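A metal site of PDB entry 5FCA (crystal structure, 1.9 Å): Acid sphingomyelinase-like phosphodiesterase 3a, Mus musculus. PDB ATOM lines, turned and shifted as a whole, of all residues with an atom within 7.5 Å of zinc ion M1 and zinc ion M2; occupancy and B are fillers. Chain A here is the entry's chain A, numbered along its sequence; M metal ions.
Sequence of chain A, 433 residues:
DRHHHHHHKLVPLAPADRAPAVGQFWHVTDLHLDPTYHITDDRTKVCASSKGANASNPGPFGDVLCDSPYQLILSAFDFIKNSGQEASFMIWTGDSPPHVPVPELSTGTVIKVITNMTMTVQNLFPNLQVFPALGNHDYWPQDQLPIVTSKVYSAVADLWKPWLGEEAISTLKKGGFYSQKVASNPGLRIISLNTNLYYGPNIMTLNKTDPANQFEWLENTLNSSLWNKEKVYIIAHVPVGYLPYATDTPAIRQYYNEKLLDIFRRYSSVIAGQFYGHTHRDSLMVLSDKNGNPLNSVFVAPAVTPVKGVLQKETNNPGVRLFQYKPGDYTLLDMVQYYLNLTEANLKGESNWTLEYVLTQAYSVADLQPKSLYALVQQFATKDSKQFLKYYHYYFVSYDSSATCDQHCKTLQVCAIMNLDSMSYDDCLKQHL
Within 4 Å of zinc ion M2: Asp 30, Asp 95, Asn 136, His 237 and His 278. The nearest printed residue that does not touch zinc ion M2 is His 137 (4.4 Å).
The side-chain carboxylate (OD1) of Asp 30 is in hydrogen-bond range of the backbone NH (N) of His 278 (2.9 Å). The backbone carbonyl oxygen (O) of Asp 30 lies within hydrogen-bond range of the backbone NH (N) of Thr 305 (3.3 Å). The backbone carbonyl oxygen (O) of Gly 94 sits at hydrogen-bond distance from the backbone NH (N) of Asp 30, 2.9 Å away. The side-chain carboxylate (OD1) of Asp 30 is in hydrogen-bond range of the side-chain hydroxyl (OG1) of Thr 29 (2.7 Å). The backbone NH (N) of Gly 277 sits at hydrogen-bond distance from the backbone carbonyl oxygen (O) of His 237, 3.1 Å away. N of Asn 136 sits at hydrogen-bond distance from OD1 of Asn 196. The backbone NH (N) of His 137 is in hydrogen-bond range of the side-chain carboxylate (OD1) of Asp 95, 2.8 Å away. The backbone carbonyl oxygen of Asp 95 lies within hydrogen-bond range of the backbone NH of Leu 31 (3.4 Å).
Within 4 Å of zinc ion M1: Asp 30, His 32, Asp 95 and His 280. The nearest printed residue that does not touch zinc ion M1 is His 278 (4.2 Å).
The side-chain carboxylate (OD2) of Asp 30 binds zinc ion M1 (2.1 Å). NE2 of His 32 binds zinc ion M1 (2.1 Å). Zinc ion M1 is bound by NE2 of His 280 (2.2 Å). OD2 of Asp 95 is bound to zinc ion M1 (2.4 Å). Zinc ion M1 has four donor atoms within binding distance.
Zinc ion M2 is bound by NE2 of His 237 (2.1 Å), OD1 of Asn 136 (2.1 Å), ND1 of His 278 (2.2 Å) and OD2 of Asp 95 (2.4 Å). Zinc ion M2 has four donor atoms within binding distance.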
ATOM      1  N   THR A  29     -13.937   8.370  -2.004  1.00  0.00           N
ATOM      2  CA  THR A  29     -13.068   7.951  -3.104  1.00  0.00           C
ATOM      3  C   THR A  29     -12.688   6.488  -2.976  1.00  0.00           C
ATOM      4  O   THR A  29     -12.673   5.941  -1.876  1.00  0.00           O
ATOM      5  CB  THR A  29     -11.798   8.832  -3.190  1.00  0.00           C
ATOM      6  OG1 THR A  29     -11.119   8.546  -4.428  1.00  0.00           O
ATOM      7  CG2 THR A  29     -10.839   8.566  -2.045  1.00  0.00           C
ATOM      8  N   ASP A  30     -12.452   5.853  -4.120  1.00  0.00           N
ATOM      9  CA  ASP A  30     -11.856   4.534  -4.179  1.00  0.00           C
ATOM     10  C   ASP A  30     -12.695   3.500  -3.408  1.00  0.00           C
ATOM     11  O   ASP A  30     -12.247   2.849  -2.454  1.00  0.00           O
ATOM     12  CB  ASP A  30     -10.423   4.587  -3.661  1.00  0.00           C
ATOM     13  CG  ASP A  30      -9.508   5.386  -4.592  1.00  0.00           C
ATOM     14  OD1 ASP A  30      -9.285   6.585  -4.313  1.00  0.00           O
ATOM     15  OD2 ASP A  30      -9.017   4.780  -5.576  1.00  0.00           O
ATOM     16  N   LEU A  31     -13.928   3.345  -3.874  1.00  0.00           N
ATOM     17  CA  LEU A  31     -14.879   2.442  -3.243  1.00  0.00           C
ATOM     18  C   LEU A  31     -14.557   0.989  -3.548  1.00  0.00           C
ATOM     19  O   LEU A  31     -14.721   0.108  -2.684  1.00  0.00           O
ATOM     20  CB  LEU A  31     -16.298   2.795  -3.714  1.00  0.00           C
ATOM     21  CG  LEU A  31     -16.766   4.222  -3.458  1.00  0.00           C
ATOM     22  CD1 LEU A  31     -18.121   4.453  -4.118  1.00  0.00           C
ATOM     23  CD2 LEU A  31     -16.835   4.463  -1.979  1.00  0.00           C
ATOM     24  N   HIS A  32     -14.149   0.704  -4.791  1.00  0.00           N
ATOM     25  CA  HIS A  32     -13.675  -0.607  -5.213  1.00  0.00           C
ATOM     26  C   HIS A  32     -14.592  -1.730  -4.715  1.00  0.00           C
ATOM     27  O   HIS A  32     -14.200  -2.629  -3.963  1.00  0.00           O
ATOM     28  CB  HIS A  32     -12.238  -0.815  -4.742  1.00  0.00           C
ATOM     29  CG  HIS A  32     -11.232   0.010  -5.476  1.00  0.00           C
ATOM     30  ND1 HIS A  32     -10.896  -0.232  -6.786  1.00  0.00           N
ATOM     31  CD2 HIS A  32     -10.445   1.043  -5.074  1.00  0.00           C
ATOM     32  CE1 HIS A  32      -9.959   0.611  -7.168  1.00  0.00           C
ATOM     33  NE2 HIS A  32      -9.665   1.388  -6.139  1.00  0.00           N
ATOM     34  N   ASP A  67     -11.105  -6.276  -1.723  1.00  0.00           N
ATOM     35  CA  ASP A  67     -11.777  -5.022  -1.959  1.00  0.00           C
ATOM     36  C   ASP A  67     -13.086  -5.005  -1.162  1.00  0.00           C
ATOM     37  O   ASP A  67     -13.370  -5.905  -0.355  1.00  0.00           O
ATOM     38  CB  ASP A  67     -11.945  -4.820  -3.449  1.00  0.00           C
ATOM     39  CG  ASP A  67     -10.815  -3.961  -4.015  1.00  0.00           C
ATOM     40  OD1 ASP A  67     -10.331  -3.066  -3.284  1.00  0.00           O
ATOM     41  OD2 ASP A  67     -10.400  -4.205  -5.170  1.00  0.00           O
ATOM     42  N   THR A  93     -14.182  10.837  -6.235  1.00  0.00           N
ATOM     43  CA  THR A  93     -13.062  10.859  -7.161  1.00  0.00           C
ATOM     44  C   THR A  93     -12.662   9.475  -7.649  1.00  0.00           C
ATOM     45  O   THR A  93     -11.492   9.227  -7.918  1.00  0.00           O
ATOM     46  CB  THR A  93     -11.876  11.605  -6.568  1.00  0.00           C
ATOM     47  OG1 THR A  93     -11.569  11.125  -5.276  1.00  0.00           O
ATOM     48  CG2 THR A  93     -12.201  13.095  -6.462  1.00  0.00           C
ATOM     49  N   GLY A  94     -13.613   8.553  -7.793  1.00  0.00           N
ATOM     50  CA  GLY A  94     -13.476   7.486  -8.783  1.00  0.00           C
ATOM     51  C   GLY A  94     -13.015   6.168  -8.193  1.00  0.00           C
ATOM     52  O   GLY A  94     -12.835   6.018  -6.992  1.00  0.00           O
ATOM     53  N   ASP A  95     -12.874   5.192  -9.103  1.00  0.00           N
ATOM     54  CA  ASP A  95     -12.346   3.827  -8.896  1.00  0.00           C
ATOM     55  C   ASP A  95     -13.351   2.846  -8.267  1.00  0.00           C
ATOM     56  O   ASP A  95     -13.248   2.460  -7.097  1.00  0.00           O
ATOM     57  CB  ASP A  95     -11.041   3.893  -8.106  1.00  0.00           C
ATOM     58  CG  ASP A  95      -9.820   3.611  -8.974  1.00  0.00           C
ATOM     59  OD1 ASP A  95      -9.866   3.672 -10.229  1.00  0.00           O
ATOM     60  OD2 ASP A  95      -8.786   3.300  -8.359  1.00  0.00           O
ATOM     61  N   SER A  96     -14.311   2.371  -9.061  1.00  0.00           N
ATOM     62  CA  SER A  96     -15.429   1.590  -8.529  1.00  0.00           C
ATOM     63  C   SER A  96     -15.257   0.092  -8.740  1.00  0.00           C
ATOM     64  O   SER A  96     -15.607  -0.680  -7.848  1.00  0.00           O
ATOM     65  CB  SER A  96     -16.748   2.096  -9.154  1.00  0.00           C
ATOM     66  OG  SER A  96     -17.100   3.359  -8.603  1.00  0.00           O
ATOM     67  N   PRO A  97     -14.782  -0.382  -9.876  1.00  0.00           N
ATOM     68  CA  PRO A  97     -14.551  -1.814 -10.005  1.00  0.00           C
ATOM     69  C   PRO A  97     -13.441  -2.280  -9.093  1.00  0.00           C
ATOM     70  O   PRO A  97     -12.624  -1.463  -8.607  1.00  0.00           O
ATOM     71  CB  PRO A  97     -14.167  -1.978 -11.486  1.00  0.00           C
ATOM     72  CG  PRO A  97     -14.770  -0.817 -12.140  1.00  0.00           C
ATOM     73  CD  PRO A  97     -14.642   0.297 -11.171  1.00  0.00           C
ATOM     74  N   HIS A  99     -10.117  -4.899  -7.789  1.00  0.00           N
ATOM     75  CA  HIS A  99      -8.817  -5.327  -8.289  1.00  0.00           C
ATOM     76  C   HIS A  99      -8.882  -6.794  -8.670  1.00  0.00           C
ATOM     77  O   HIS A  99      -8.523  -7.678  -7.882  1.00  0.00           O
ATOM     78  CB  HIS A  99      -7.741  -5.075  -7.233  1.00  0.00           C
ATOM     79  CG  HIS A  99      -7.465  -3.620  -6.981  1.00  0.00           C
ATOM     80  ND1 HIS A  99      -8.205  -2.866  -6.112  1.00  0.00           N
ATOM     81  CD2 HIS A  99      -6.539  -2.795  -7.521  1.00  0.00           C
ATOM     82  CE1 HIS A  99      -7.734  -1.626  -6.089  1.00  0.00           C
ATOM     83  NE2 HIS A  99      -6.718  -1.567  -6.940  1.00  0.00           N
ATOM     84  N   LEU A 134     -13.543  10.172 -12.970  1.00  0.00           N
ATOM     85  CA  LEU A 134     -13.225   8.800 -13.312  1.00  0.00           C
ATOM     86  C   LEU A 134     -11.876   8.404 -12.731  1.00  0.00           C
ATOM     87  O   LEU A 134     -10.944   9.206 -12.640  1.00  0.00           O
ATOM     88  CB  LEU A 134     -13.207   8.612 -14.830  1.00  0.00           C
ATOM     89  CG  LEU A 134     -14.520   8.781 -15.567  1.00  0.00           C
ATOM     90  CD1 LEU A 134     -14.237   8.998 -17.052  1.00  0.00           C
ATOM     91  CD2 LEU A 134     -15.381   7.526 -15.344  1.00  0.00           C
ATOM     92  N   GLY A 135     -11.791   7.127 -12.326  1.00  0.00           N
ATOM     93  CA  GLY A 135     -10.582   6.516 -11.841  1.00  0.00           C
ATOM     94  C   GLY A 135      -9.997   5.568 -12.856  1.00  0.00           C
ATOM     95  O   GLY A 135     -10.604   5.254 -13.874  1.00  0.00           O
ATOM     96  N   ASN A 136      -8.748   5.127 -12.598  1.00  0.00           N
ATOM     97  CA  ASN A 136      -8.077   4.312 -13.603  1.00  0.00           C
ATOM     98  C   ASN A 136      -8.702   2.927 -13.719  1.00  0.00           C
ATOM     99  O   ASN A 136      -8.549   2.265 -14.759  1.00  0.00           O
ATOM    100  CB  ASN A 136      -6.579   4.195 -13.295  1.00  0.00           C
ATOM    101  CG  ASN A 136      -6.309   3.676 -11.909  1.00  0.00           C
ATOM    102  OD1 ASN A 136      -6.693   4.282 -10.927  1.00  0.00           O
ATOM    103  ND2 ASN A 136      -5.649   2.537 -11.829  1.00  0.00           N
ATOM    104  N   HIS A 137      -9.424   2.492 -12.707  1.00  0.00           N
ATOM    105  CA  HIS A 137     -10.181   1.250 -12.759  1.00  0.00           C
ATOM    106  C   HIS A 137     -11.567   1.421 -13.352  1.00  0.00           C
ATOM    107  O   HIS A 137     -12.270   0.417 -13.550  1.00  0.00           O
ATOM    108  CB  HIS A 137     -10.279   0.678 -11.344  1.00  0.00           C
ATOM    109  CG  HIS A 137      -9.021   0.020 -10.894  1.00  0.00           C
ATOM    110  ND1 HIS A 137      -8.653  -1.227 -11.325  1.00  0.00           N
ATOM    111  CD2 HIS A 137      -8.038   0.454 -10.063  1.00  0.00           C
ATOM    112  CE1 HIS A 137      -7.501  -1.552 -10.767  1.00  0.00           C
ATOM    113  NE2 HIS A 137      -7.108  -0.562  -9.987  1.00  0.00           N
ATOM    114  N   ASP A 138     -11.973   2.648 -13.675  1.00  0.00           N
ATOM    115  CA  ASP A 138     -13.285   2.908 -14.266  1.00  0.00           C
ATOM    116  C   ASP A 138     -13.267   2.760 -15.772  1.00  0.00           C
ATOM    117  O   ASP A 138     -13.828   3.588 -16.493  1.00  0.00           O
ATOM    118  CB  ASP A 138     -13.762   4.309 -13.839  1.00  0.00           C
ATOM    119  CG  ASP A 138     -14.065   4.371 -12.343  1.00  0.00           C
ATOM    120  OD1 ASP A 138     -14.334   3.309 -11.753  1.00  0.00           O
ATOM    121  OD2 ASP A 138     -14.041   5.472 -11.756  1.00  0.00           O
ATOM    122  N   ASP A 143      -6.908   1.225 -16.669  1.00  0.00           N
ATOM    123  CA  ASP A 143      -5.871   2.209 -16.962  1.00  0.00           C
ATOM    124  C   ASP A 143      -5.859   2.702 -18.409  1.00  0.00           C
ATOM    125  O   ASP A 143      -5.186   3.690 -18.708  1.00  0.00           O
ATOM    126  CB  ASP A 143      -4.471   1.644 -16.660  1.00  0.00           C
ATOM    127  CG  ASP A 143      -4.328   1.041 -15.269  1.00  0.00           C
ATOM    128  OD1 ASP A 143      -4.943   1.526 -14.306  1.00  0.00           O
ATOM    129  OD2 ASP A 143      -3.564   0.061 -15.146  1.00  0.00           O
ATOM    130  N   ASN A 196      -6.220  10.179 -15.289  1.00  0.00           N
ATOM    131  CA  ASN A 196      -5.847   8.897 -15.842  1.00  0.00           C
ATOM    132  C   ASN A 196      -5.268   9.007 -17.244  1.00  0.00           C
ATOM    133  O   ASN A 196      -4.581   8.072 -17.683  1.00  0.00           O
ATOM    134  CB  ASN A 196      -7.055   7.979 -15.868  1.00  0.00           C
ATOM    135  CG  ASN A 196      -7.757   7.966 -14.572  1.00  0.00           C
ATOM    136  OD1 ASN A 196      -7.255   7.413 -13.594  1.00  0.00           O
ATOM    137  ND2 ASN A 196      -8.871   8.676 -14.494  1.00  0.00           N
ATOM    138  N   TYR A 199      -1.567   8.887 -16.548  1.00  0.00           N
ATOM    139  CA  TYR A 199      -1.102   7.826 -15.666  1.00  0.00           C
ATOM    140  C   TYR A 199      -0.218   6.853 -16.431  1.00  0.00           C
ATOM    141  O   TYR A 199      -0.519   6.473 -17.570  1.00  0.00           O
ATOM    142  CB  TYR A 199      -2.329   7.138 -15.045  1.00  0.00           C
ATOM    143  CG  TYR A 199      -2.064   6.084 -13.980  1.00  0.00           C
ATOM    144  CD1 TYR A 199      -1.203   6.316 -12.939  1.00  0.00           C
ATOM    145  CD2 TYR A 199      -2.731   4.865 -14.017  1.00  0.00           C
ATOM    146  CE1 TYR A 199      -0.984   5.367 -11.972  1.00  0.00           C
ATOM    147  CE2 TYR A 199      -2.505   3.893 -13.048  1.00  0.00           C
ATOM    148  CZ  TYR A 199      -1.622   4.159 -12.030  1.00  0.00           C
ATOM    149  OH  TYR A 199      -1.346   3.218 -11.042  1.00  0.00           O
ATOM    150  N   HIS A 237      -8.757  11.848 -10.009  1.00  0.00           N
ATOM    151  CA  HIS A 237      -8.373  10.600  -9.375  1.00  0.00           C
ATOM    152  C   HIS A 237      -6.892  10.554  -9.027  1.00  0.00           C
ATOM    153  O   HIS A 237      -6.528  10.634  -7.853  1.00  0.00           O
ATOM    154  CB  HIS A 237      -8.720   9.409 -10.258  1.00  0.00           C
ATOM    155  CG  HIS A 237      -8.550   8.110  -9.544  1.00  0.00           C
ATOM    156  ND1 HIS A 237      -9.175   7.836  -8.355  1.00  0.00           N
ATOM    157  CD2 HIS A 237      -7.768   7.032  -9.813  1.00  0.00           C
ATOM    158  CE1 HIS A 237      -8.808   6.641  -7.926  1.00  0.00           C
ATOM    159  NE2 HIS A 237      -7.960   6.138  -8.800  1.00  0.00           N
ATOM    160  N   VAL A 238      -6.019  10.379 -10.025  1.00  0.00           N
ATOM    161  CA  VAL A 238      -4.572  10.315  -9.756  1.00  0.00           C
ATOM    162  C   VAL A 238      -4.058  11.705  -9.421  1.00  0.00           C
ATOM    163  O   VAL A 238      -4.339  12.671 -10.170  1.00  0.00           O
ATOM    164  CB  VAL A 238      -3.824   9.757 -10.964  1.00  0.00           C
ATOM    165  CG1 VAL A 238      -2.343   9.563 -10.584  1.00  0.00           C
ATOM    166  CG2 VAL A 238      -4.433   8.465 -11.438  1.00  0.00           C
ATOM    167  N   GLY A 277      -7.662  11.263  -5.087  1.00  0.00           N
ATOM    168  CA  GLY A 277      -7.598   9.979  -4.403  1.00  0.00           C
ATOM    169  C   GLY A 277      -6.521   9.088  -4.960  1.00  0.00           C
ATOM    170  O   GLY A 277      -5.356   9.460  -5.034  1.00  0.00           O
ATOM    171  N   HIS A 278      -6.908   7.906  -5.406  1.00  0.00           N
ATOM    172  CA  HIS A 278      -6.047   6.927  -6.050  1.00  0.00           C
ATOM    173  C   HIS A 278      -4.995   6.286  -5.146  1.00  0.00           C
ATOM    174  O   HIS A 278      -4.710   5.089  -5.294  1.00  0.00           O
ATOM    175  CB  HIS A 278      -5.324   7.516  -7.263  1.00  0.00           C
ATOM    176  CG  HIS A 278      -4.387   6.576  -7.897  1.00  0.00           C
ATOM    177  ND1 HIS A 278      -4.797   5.481  -8.636  1.00  0.00           N
ATOM    178  CD2 HIS A 278      -3.027   6.539  -7.913  1.00  0.00           C
ATOM    179  CE1 HIS A 278      -3.747   4.832  -9.089  1.00  0.00           C
ATOM    180  NE2 HIS A 278      -2.666   5.451  -8.666  1.00  0.00           N
ATOM    181  N   THR A 279      -4.393   7.041  -4.239  1.00  0.00           N
ATOM    182  CA  THR A 279      -3.327   6.434  -3.436  1.00  0.00           C
ATOM    183  C   THR A 279      -3.858   5.600  -2.288  1.00  0.00           C
ATOM    184  O   THR A 279      -3.110   4.811  -1.723  1.00  0.00           O
ATOM    185  CB  THR A 279      -2.403   7.491  -2.838  1.00  0.00           C
ATOM    186  OG1 THR A 279      -3.093   8.202  -1.822  1.00  0.00           O
ATOM    187  CG2 THR A 279      -1.881   8.490  -3.849  1.00  0.00           C
ATOM    188  N   HIS A 280      -5.112   5.797  -1.892  1.00  0.00           N
ATOM    189  CA  HIS A 280      -5.736   5.094  -0.768  1.00  0.00           C
ATOM    190  C   HIS A 280      -5.134   5.487   0.564  1.00  0.00           C
ATOM    191  O   HIS A 280      -5.264   4.756   1.538  1.00  0.00           O
ATOM    192  CB  HIS A 280      -5.651   3.571  -0.936  1.00  0.00           C
ATOM    193  CG  HIS A 280      -6.409   3.038  -2.113  1.00  0.00           C
ATOM    194  ND1 HIS A 280      -6.765   1.711  -2.222  1.00  0.00           N
ATOM    195  CD2 HIS A 280      -6.871   3.647  -3.232  1.00  0.00           C
ATOM    196  CE1 HIS A 280      -7.410   1.524  -3.367  1.00  0.00           C
ATOM    197  NE2 HIS A 280      -7.474   2.680  -3.999  1.00  0.00           N
ATOM    198  N   ALA A 303      -9.022   5.773   0.936  1.00  0.00           N
ATOM    199  CA  ALA A 303     -10.057   4.997   0.281  1.00  0.00           C
ATOM    200  C   ALA A 303     -11.017   4.390   1.304  1.00  0.00           C
ATOM    201  O   ALA A 303     -10.683   4.179   2.470  1.00  0.00           O
ATOM    202  CB  ALA A 303      -9.433   3.897  -0.555  1.00  0.00           C
ATOM    203  N   THR A 305     -12.169   1.266   0.434  1.00  0.00           N
ATOM    204  CA  THR A 305     -11.612  -0.076   0.406  1.00  0.00           C
ATOM    205  C   THR A 305     -10.356  -0.141   1.261  1.00  0.00           C
ATOM    206  O   THR A 305      -9.611   0.845   1.349  1.00  0.00           O
ATOM    207  CB  THR A 305     -11.284  -0.524  -1.011  1.00  0.00           C
ATOM    208  OG1 THR A 305     -10.932  -1.906  -0.968  1.00  0.00           O
ATOM    209  CG2 THR A 305     -10.103   0.268  -1.603  1.00  0.00           C
ATOM    210  N   VAL A 307      -8.081  -2.638   0.724  1.00  0.00           N
ATOM    211  CA  VAL A 307      -7.328  -3.701   0.074  1.00  0.00           C
ATOM    212  C   VAL A 307      -5.840  -3.393   0.062  1.00  0.00           C
ATOM    213  O   VAL A 307      -5.421  -2.236  -0.069  1.00  0.00           O
ATOM    214  CB  VAL A 307      -7.864  -3.911  -1.343  1.00  0.00           C
ATOM    215  CG1 VAL A 307      -7.447  -2.732  -2.268  1.00  0.00           C
ATOM    216  CG2 VAL A 307      -7.413  -5.254  -1.899  1.00  0.00           C
HETATM  217 ZN    ZN M   1      -8.243   2.920  -6.015  1.00  0.00          ZN
HETATM  218 ZN    ZN M   2      -6.738   4.428  -8.829  1.00  0.00          ZN
HETATM  219 ZN    ZN M   3      -5.348   0.482  -8.245  1.00  0.00          ZN
